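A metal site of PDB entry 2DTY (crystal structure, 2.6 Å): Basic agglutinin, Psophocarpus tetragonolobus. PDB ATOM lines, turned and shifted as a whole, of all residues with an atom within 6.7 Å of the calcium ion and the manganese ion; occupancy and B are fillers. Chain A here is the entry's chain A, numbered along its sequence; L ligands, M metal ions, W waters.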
ATOM      1  N   ASP A  87       0.918  -7.915  -1.339  1.00  0.00           N
ATOM      2  CA  ASP A  87       1.406  -6.593  -0.943  1.00  0.00           C
ATOM      3  C   ASP A  87       0.307  -5.527  -1.099  1.00  0.00           C
ATOM      4  O   ASP A  87       0.313  -4.489  -0.430  1.00  0.00           O
ATOM      5  CB  ASP A  87       2.598  -6.179  -1.811  1.00  0.00           C
ATOM      6  CG  ASP A  87       3.920  -6.775  -1.345  1.00  0.00           C
ATOM      7  OD1 ASP A  87       4.267  -7.903  -1.763  1.00  0.00           O
ATOM      8  OD2 ASP A  87       4.599  -6.101  -0.540  1.00  0.00           O
ATOM      9  N   GLY A 104       6.432  -7.242  -5.534  1.00  0.00           N
ATOM     10  CA  GLY A 104       6.528  -6.957  -4.123  1.00  0.00           C
ATOM     11  C   GLY A 104       6.005  -5.591  -3.760  1.00  0.00           C
ATOM     12  O   GLY A 104       4.966  -5.169  -4.254  1.00  0.00           O
ATOM     13  N   GLY A 105       6.739  -4.890  -2.893  1.00  0.00           N
ATOM     14  CA  GLY A 105       6.335  -3.575  -2.457  1.00  0.00           C
ATOM     15  C   GLY A 105       6.177  -2.551  -3.558  1.00  0.00           C
ATOM     16  O   GLY A 105       5.656  -1.466  -3.330  1.00  0.00           O
ATOM     17  N   TYR A 106       6.627  -2.882  -4.772  1.00  0.00           N
ATOM     18  CA  TYR A 106       6.515  -1.953  -5.882  1.00  0.00           C
ATOM     19  C   TYR A 106       5.254  -2.173  -6.734  1.00  0.00           C
ATOM     20  O   TYR A 106       5.043  -1.473  -7.744  1.00  0.00           O
ATOM     21  CB  TYR A 106       7.787  -2.007  -6.725  1.00  0.00           C
ATOM     22  CG  TYR A 106       9.008  -1.494  -5.961  1.00  0.00           C
ATOM     23  CD1 TYR A 106       9.043  -0.192  -5.461  1.00  0.00           C
ATOM     24  CD2 TYR A 106      10.096  -2.322  -5.699  1.00  0.00           C
ATOM     25  CE1 TYR A 106      10.134   0.277  -4.738  1.00  0.00           C
ATOM     26  CE2 TYR A 106      11.196  -1.862  -4.971  1.00  0.00           C
ATOM     27  CZ  TYR A 106      11.205  -0.560  -4.488  1.00  0.00           C
ATOM     28  OH  TYR A 106      12.283  -0.101  -3.762  1.00  0.00           O
ATOM     29  N   PHE A 107       4.419  -3.120  -6.312  1.00  0.00           N
ATOM     30  CA  PHE A 107       3.138  -3.415  -6.969  1.00  0.00           C
ATOM     31  C   PHE A 107       3.188  -3.714  -8.471  1.00  0.00           C
ATOM     32  O   PHE A 107       2.148  -3.867  -9.106  1.00  0.00           O
ATOM     33  CB  PHE A 107       2.176  -2.242  -6.771  1.00  0.00           C
ATOM     34  CG  PHE A 107       2.045  -1.793  -5.350  1.00  0.00           C
ATOM     35  CD1 PHE A 107       1.430  -2.593  -4.408  1.00  0.00           C
ATOM     36  CD2 PHE A 107       2.478  -0.529  -4.975  1.00  0.00           C
ATOM     37  CE1 PHE A 107       1.246  -2.142  -3.077  1.00  0.00           C
ATOM     38  CE2 PHE A 107       2.301  -0.073  -3.667  1.00  0.00           C
ATOM     39  CZ  PHE A 107       1.685  -0.880  -2.718  1.00  0.00           C
ATOM     40  N   GLU A 122      -2.985   3.691  -4.264  1.00  0.00           N
ATOM     41  CA  GLU A 122      -2.686   2.376  -3.735  1.00  0.00           C
ATOM     42  C   GLU A 122      -3.511   1.955  -2.526  1.00  0.00           C
ATOM     43  O   GLU A 122      -3.992   2.769  -1.738  1.00  0.00           O
ATOM     44  CB  GLU A 122      -1.215   2.297  -3.339  1.00  0.00           C
ATOM     45  CG  GLU A 122      -0.910   3.141  -2.109  1.00  0.00           C
ATOM     46  CD  GLU A 122       0.476   2.896  -1.547  1.00  0.00           C
ATOM     47  OE1 GLU A 122       1.476   3.204  -2.235  1.00  0.00           O
ATOM     48  OE2 GLU A 122       0.576   2.406  -0.412  1.00  0.00           O
ATOM     49  N   ASP A 124      -2.429  -0.462   0.088  1.00  0.00           N
ATOM     50  CA  ASP A 124      -1.266  -1.157   0.639  1.00  0.00           C
ATOM     51  C   ASP A 124      -1.553  -2.033   1.846  1.00  0.00           C
ATOM     52  O   ASP A 124      -2.026  -1.555   2.864  1.00  0.00           O
ATOM     53  CB  ASP A 124      -0.214  -0.122   1.025  1.00  0.00           C
ATOM     54  CG  ASP A 124       1.191  -0.659   0.947  1.00  0.00           C
ATOM     55  OD1 ASP A 124       1.373  -1.894   1.058  1.00  0.00           O
ATOM     56  OD2 ASP A 124       2.120   0.156   0.772  1.00  0.00           O
ATOM     57  N   THR A 125      -1.226  -3.311   1.719  1.00  0.00           N
ATOM     58  CA  THR A 125      -1.460  -4.270   2.801  1.00  0.00           C
ATOM     59  C   THR A 125      -0.199  -4.699   3.566  1.00  0.00           C
ATOM     60  O   THR A 125      -0.305  -5.290   4.637  1.00  0.00           O
ATOM     61  CB  THR A 125      -2.184  -5.506   2.244  1.00  0.00           C
ATOM     62  OG1 THR A 125      -1.455  -6.016   1.125  1.00  0.00           O
ATOM     63  CG2 THR A 125      -3.600  -5.119   1.785  1.00  0.00           C
ATOM     64  N   PHE A 126       0.975  -4.414   3.013  1.00  0.00           N
ATOM     65  CA  PHE A 126       2.239  -4.771   3.652  1.00  0.00           C
ATOM     66  C   PHE A 126       3.051  -3.530   3.987  1.00  0.00           C
ATOM     67  O   PHE A 126       3.145  -2.590   3.196  1.00  0.00           O
ATOM     68  CB  PHE A 126       3.065  -5.650   2.734  1.00  0.00           C
ATOM     69  CG  PHE A 126       4.381  -6.037   3.316  1.00  0.00           C
ATOM     70  CD1 PHE A 126       4.470  -7.076   4.236  1.00  0.00           C
ATOM     71  CD2 PHE A 126       5.542  -5.335   2.997  1.00  0.00           C
ATOM     72  CE1 PHE A 126       5.688  -7.404   4.828  1.00  0.00           C
ATOM     73  CE2 PHE A 126       6.758  -5.655   3.569  1.00  0.00           C
ATOM     74  CZ  PHE A 126       6.837  -6.691   4.490  1.00  0.00           C
ATOM     75  N   ARG A 127       3.660  -3.530   5.168  1.00  0.00           N
ATOM     76  CA  ARG A 127       4.455  -2.389   5.602  1.00  0.00           C
ATOM     77  C   ARG A 127       5.940  -2.470   5.240  1.00  0.00           C
ATOM     78  O   ARG A 127       6.703  -3.164   5.907  1.00  0.00           O
ATOM     79  CB  ARG A 127       4.301  -2.198   7.112  1.00  0.00           C
ATOM     80  CG  ARG A 127       4.897  -0.894   7.628  1.00  0.00           C
ATOM     81  CD  ARG A 127       4.499  -0.601   9.067  1.00  0.00           C
ATOM     82  NE  ARG A 127       5.001   0.709   9.496  1.00  0.00           N
ATOM     83  CZ  ARG A 127       4.820   1.233  10.700  1.00  0.00           C
ATOM     84  NH1 ARG A 127       4.143   0.562  11.628  1.00  0.00           N
ATOM     85  NH2 ARG A 127       5.297   2.433  10.982  1.00  0.00           N
ATOM     86  N   ASN A 128       6.345  -1.755   4.193  1.00  0.00           N
ATOM     87  CA  ASN A 128       7.740  -1.720   3.800  1.00  0.00           C
ATOM     88  C   ASN A 128       8.470  -0.685   4.640  1.00  0.00           C
ATOM     89  O   ASN A 128       7.865   0.025   5.441  1.00  0.00           O
ATOM     90  CB  ASN A 128       7.898  -1.351   2.326  1.00  0.00           C
ATOM     91  CG  ASN A 128       7.450  -2.447   1.401  1.00  0.00           C
ATOM     92  OD1 ASN A 128       6.256  -2.577   1.127  1.00  0.00           O
ATOM     93  ND2 ASN A 128       8.390  -3.266   0.933  1.00  0.00           N
ATOM     94  N   TRP A 130       9.494   2.095   3.922  1.00  0.00           N
ATOM     95  CA  TRP A 130       9.017   3.449   3.637  1.00  0.00           C
ATOM     96  C   TRP A 130       7.533   3.677   3.906  1.00  0.00           C
ATOM     97  O   TRP A 130       7.003   4.743   3.577  1.00  0.00           O
ATOM     98  CB  TRP A 130       9.303   3.772   2.169  1.00  0.00           C
ATOM     99  CG  TRP A 130       8.622   2.804   1.229  1.00  0.00           C
ATOM    100  CD1 TRP A 130       7.290   2.738   0.925  1.00  0.00           C
ATOM    101  CD2 TRP A 130       9.244   1.727   0.509  1.00  0.00           C
ATOM    102  NE1 TRP A 130       7.043   1.691   0.067  1.00  0.00           N
ATOM    103  CE2 TRP A 130       8.221   1.045  -0.201  1.00  0.00           C
ATOM    104  CE3 TRP A 130      10.565   1.259   0.396  1.00  0.00           C
ATOM    105  CZ2 TRP A 130       8.481  -0.064  -1.012  1.00  0.00           C
ATOM    106  CZ3 TRP A 130      10.821   0.144  -0.422  1.00  0.00           C
ATOM    107  CH2 TRP A 130       9.781  -0.503  -1.111  1.00  0.00           C
ATOM    108  N   ASP A 131       6.864   2.687   4.499  1.00  0.00           N
ATOM    109  CA  ASP A 131       5.421   2.756   4.779  1.00  0.00           C
ATOM    110  C   ASP A 131       5.034   3.023   6.206  1.00  0.00           C
ATOM    111  O   ASP A 131       5.786   2.731   7.134  1.00  0.00           O
ATOM    112  CB  ASP A 131       4.721   1.431   4.436  1.00  0.00           C
ATOM    113  CG  ASP A 131       4.503   1.219   2.961  1.00  0.00           C
ATOM    114  OD1 ASP A 131       4.157   2.187   2.266  1.00  0.00           O
ATOM    115  OD2 ASP A 131       4.661   0.066   2.502  1.00  0.00           O
ATOM    116  N   PRO A 132       3.840   3.601   6.401  1.00  0.00           N
ATOM    117  CA  PRO A 132       3.298   3.900   7.719  1.00  0.00           C
ATOM    118  C   PRO A 132       2.452   2.669   8.044  1.00  0.00           C
ATOM    119  O   PRO A 132       2.412   1.738   7.237  1.00  0.00           O
ATOM    120  CB  PRO A 132       2.452   5.135   7.469  1.00  0.00           C
ATOM    121  CG  PRO A 132       1.920   4.883   6.117  1.00  0.00           C
ATOM    122  CD  PRO A 132       3.154   4.405   5.377  1.00  0.00           C
ATOM    123  N   ILE A 134      -0.141  -0.240   8.214  1.00  0.00           N
ATOM    124  CA  ILE A 134      -0.997  -0.764   7.146  1.00  0.00           C
ATOM    125  C   ILE A 134      -2.228  -1.424   7.751  1.00  0.00           C
ATOM    126  O   ILE A 134      -2.250  -1.774   8.921  1.00  0.00           O
ATOM    127  CB  ILE A 134      -0.245  -1.806   6.254  1.00  0.00           C
ATOM    128  CG1 ILE A 134       0.434  -2.896   7.109  1.00  0.00           C
ATOM    129  CG2 ILE A 134       0.811  -1.094   5.429  1.00  0.00           C
ATOM    130  CD1 ILE A 134      -0.514  -3.928   7.708  1.00  0.00           C
ATOM    131  N   HIS A 136      -3.383   0.914   4.292  1.00  0.00           N
ATOM    132  CA  HIS A 136      -3.597   2.328   4.091  1.00  0.00           C
ATOM    133  C   HIS A 136      -3.820   2.664   2.625  1.00  0.00           C
ATOM    134  O   HIS A 136      -3.376   1.950   1.735  1.00  0.00           O
ATOM    135  CB  HIS A 136      -2.418   3.148   4.653  1.00  0.00           C
ATOM    136  CG  HIS A 136      -1.088   2.804   4.061  1.00  0.00           C
ATOM    137  ND1 HIS A 136      -0.116   2.107   4.755  1.00  0.00           N
ATOM    138  CD2 HIS A 136      -0.545   3.073   2.845  1.00  0.00           C
ATOM    139  CE1 HIS A 136       0.964   1.978   4.006  1.00  0.00           C
ATOM    140  NE2 HIS A 136       0.730   2.545   2.840  1.00  0.00           N
ATOM    141  N   ILE A 137      -4.546   3.752   2.390  1.00  0.00           N
ATOM    142  CA  ILE A 137      -4.803   4.237   1.050  1.00  0.00           C
ATOM    143  C   ILE A 137      -3.670   5.213   0.856  1.00  0.00           C
ATOM    144  O   ILE A 137      -3.241   5.858   1.814  1.00  0.00           O
ATOM    145  CB  ILE A 137      -6.104   5.032   0.970  1.00  0.00           C
ATOM    146  CG1 ILE A 137      -7.270   4.176   1.461  1.00  0.00           C
ATOM    147  CG2 ILE A 137      -6.350   5.470  -0.449  1.00  0.00           C
ATOM    148  CD1 ILE A 137      -8.598   4.897   1.447  1.00  0.00           C
ATOM    149  N   GLY A 138      -3.162   5.330  -0.362  1.00  0.00           N
ATOM    150  CA  GLY A 138      -2.079   6.261  -0.577  1.00  0.00           C
ATOM    151  C   GLY A 138      -2.082   6.789  -1.984  1.00  0.00           C
ATOM    152  O   GLY A 138      -2.469   6.095  -2.932  1.00  0.00           O
ATOM    153  N   ASP A 140       0.234   8.052  -4.878  1.00  0.00           N
ATOM    154  CA  ASP A 140       1.611   8.004  -5.330  1.00  0.00           C
ATOM    155  C   ASP A 140       1.834   8.744  -6.641  1.00  0.00           C
ATOM    156  O   ASP A 140       1.064   8.600  -7.594  1.00  0.00           O
ATOM    157  CB  ASP A 140       2.070   6.553  -5.497  1.00  0.00           C
ATOM    158  CG  ASP A 140       1.798   5.717  -4.276  1.00  0.00           C
ATOM    159  OD1 ASP A 140       1.735   6.279  -3.166  1.00  0.00           O
ATOM    160  OD2 ASP A 140       1.644   4.487  -4.419  1.00  0.00           O
ATOM    161  N   VAL A 144       6.596   5.009  -5.081  1.00  0.00           N
ATOM    162  CA  VAL A 144       5.725   4.219  -4.236  1.00  0.00           C
ATOM    163  C   VAL A 144       5.732   4.775  -2.823  1.00  0.00           C
ATOM    164  O   VAL A 144       5.095   4.226  -1.925  1.00  0.00           O
ATOM    165  CB  VAL A 144       6.154   2.756  -4.244  1.00  0.00           C
ATOM    166  CG1 VAL A 144       7.391   2.562  -3.378  1.00  0.00           C
ATOM    167  CG2 VAL A 144       5.006   1.887  -3.794  1.00  0.00           C
ATOM    168  N   ILE A 145       6.468   5.861  -2.612  1.00  0.00           N
ATOM    169  CA  ILE A 145       6.505   6.482  -1.289  1.00  0.00           C
ATOM    170  C   ILE A 145       5.500   7.646  -1.350  1.00  0.00           C
ATOM    171  O   ILE A 145       5.824   8.760  -1.751  1.00  0.00           O
ATOM    172  CB  ILE A 145       7.922   6.981  -0.945  1.00  0.00           C
ATOM    173  CG1 ILE A 145       7.916   7.688   0.408  1.00  0.00           C
ATOM    174  CG2 ILE A 145       8.433   7.915  -2.000  1.00  0.00           C
ATOM    175  CD1 ILE A 145       9.282   8.194   0.844  1.00  0.00           C
ATOM    176  N   SER A 146       4.268   7.326  -0.953  1.00  0.00           N
ATOM    177  CA  SER A 146       3.107   8.227  -0.984  1.00  0.00           C
ATOM    178  C   SER A 146       3.248   9.652  -0.507  1.00  0.00           C
ATOM    179  O   SER A 146       3.980   9.933   0.427  1.00  0.00           O
ATOM    180  CB  SER A 146       1.964   7.577  -0.201  1.00  0.00           C
ATOM    181  OG  SER A 146       1.761   6.244  -0.645  1.00  0.00           O
ATOM    182  N   THR A 149      -1.342   9.812   2.922  1.00  0.00           N
ATOM    183  CA  THR A 149      -1.724   8.479   3.350  1.00  0.00           C
ATOM    184  C   THR A 149      -2.833   8.498   4.388  1.00  0.00           C
ATOM    185  O   THR A 149      -2.918   9.414   5.185  1.00  0.00           O
ATOM    186  CB  THR A 149      -0.492   7.733   3.941  1.00  0.00           C
ATOM    187  OG1 THR A 149       0.260   7.142   2.884  1.00  0.00           O
ATOM    188  CG2 THR A 149      -0.909   6.675   4.917  1.00  0.00           C
HETATM  189  O1  LIG L   1       9.058  -9.302   1.004  1.00  0.00           O
HETATM  190  C1  LIG L   1       9.960  -8.132   0.764  1.00  0.00           C
HETATM  191  O2  LIG L   1      10.372  -7.498   1.986  1.00  0.00           O
HETATM  192  C2  LIG L   1       9.215  -7.096  -0.166  1.00  0.00           C
HETATM  193  N1  LIG L   1      10.066  -5.933  -0.388  1.00  0.00           N
HETATM  194  C3  LIG L   1       7.843  -6.695   0.497  1.00  0.00           C
HETATM  195  O3  LIG L   1       7.167  -5.761  -0.332  1.00  0.00           O
HETATM  196  C4  LIG L   1       6.980  -7.958   0.700  1.00  0.00           C
HETATM  197  O4  LIG L   1       6.665  -8.555  -0.562  1.00  0.00           O
HETATM  198  C5  LIG L   1       7.749  -8.957   1.599  1.00  0.00           C
HETATM  199  C6  LIG L   1       6.957 -10.242   1.815  1.00  0.00           C
HETATM  200  O5  LIG L   1       7.485 -11.080   2.848  1.00  0.00           O
HETATM  201  C7  LIG L   1      10.225  -5.373  -1.603  1.00  0.00           C
HETATM  202  O6  LIG L   1       9.680  -5.776  -2.636  1.00  0.00           O
HETATM  203  C8  LIG L   1      11.141  -4.155  -1.661  1.00  0.00           C
HETATM  204 CA    CA M   1       3.884  -1.677   1.133  1.00  0.00          CA
HETATM  205 MN    MN M   2       2.282   2.461   1.086  1.00  0.00          MN
HETATM  206  O   HOH W   1       3.488  -3.519  -0.397  1.00  0.00           O
HETATM  207  O   HOH W   2       2.909   4.724   1.247  1.00  0.00           O
HETATM  208  O   HOH W   3       4.759  -0.554  -0.887  1.00  0.00           O
HETATM  209  O   HOH W   4       3.742   2.052  -0.872  1.00  0.00           O
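ND2 of Asn 128 lies within hydrogen-bond range of O3 of the ligand (3.1 Å). An oxygen (O3) of the ligand sits at hydrogen-bond distance from the backbone NH (N) of Gly 105, 2.7 Å away. The side-chain carboxylate (OD2) of Asp 87 lies within hydrogen-bond range of an oxygen (O3) of the ligand, at 2.6 Å.
Along chain A the residues within 4 Å of the calcium ion span positions 124 to 131.
Water W3 lies within hydrogen-bond range of O of Gly 105 (2.8 Å) and NE1 of Trp 130 (3.3 Å). Water W4 lies within hydrogen-bond range of the backbone carbonyl oxygen (O) of Val 144 (2.8 Å), the side-chain carboxylate (OE1) of Glu 122 (2.9 Å) and the indole nitrogen (NE1) of Trp 130 (3.5 Å).
Along chain A the residues within 4 Å of the manganese ion span positions 122 to 136. The nearest printed residue that does not touch the manganese ion is Ser 146 (4.2 Å).
The calcium ion is bound by OD2 of Asp 131 (2.3 Å), O of Phe 126 (2.4 Å), water W1 (2.4 Å), water W3 (2.5 Å), OD1 of Asp 124 (2.5 Å), OD1 of Asn 128 (2.5 Å) and OD2 of Asp 124 (2.6 Å). The calcium ion has seven donor atoms within binding distance.
The manganese ion is bound by OD1 of Asp 131 (2.2 Å), OE2 of Glu 122 (2.3 Å), OD2 of Asp 124 (2.3 Å), NE2 of His 136 (2.3 Å), water W2 (2.4 Å) and water W4 (2.5 Å). The manganese ion has six donor atoms within binding distance.
The backbone carbonyl oxygen of Asp 131 lies within hydrogen-bond range of the guanidinium group of Arg 127 (3.2 Å). The side-chain hydroxyl of Ser 146 lies within hydrogen-bond range of the side-chain carboxylate of Glu 122, 3.4 Å away. OE1 of Glu 122 lies close to OD2 of Asp 140, at 2.5 Å. The backbone NH (N) of Glu 122 lies within hydrogen-bond range of the backbone carbonyl oxygen (O) of Gly 138 (2.8 Å).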
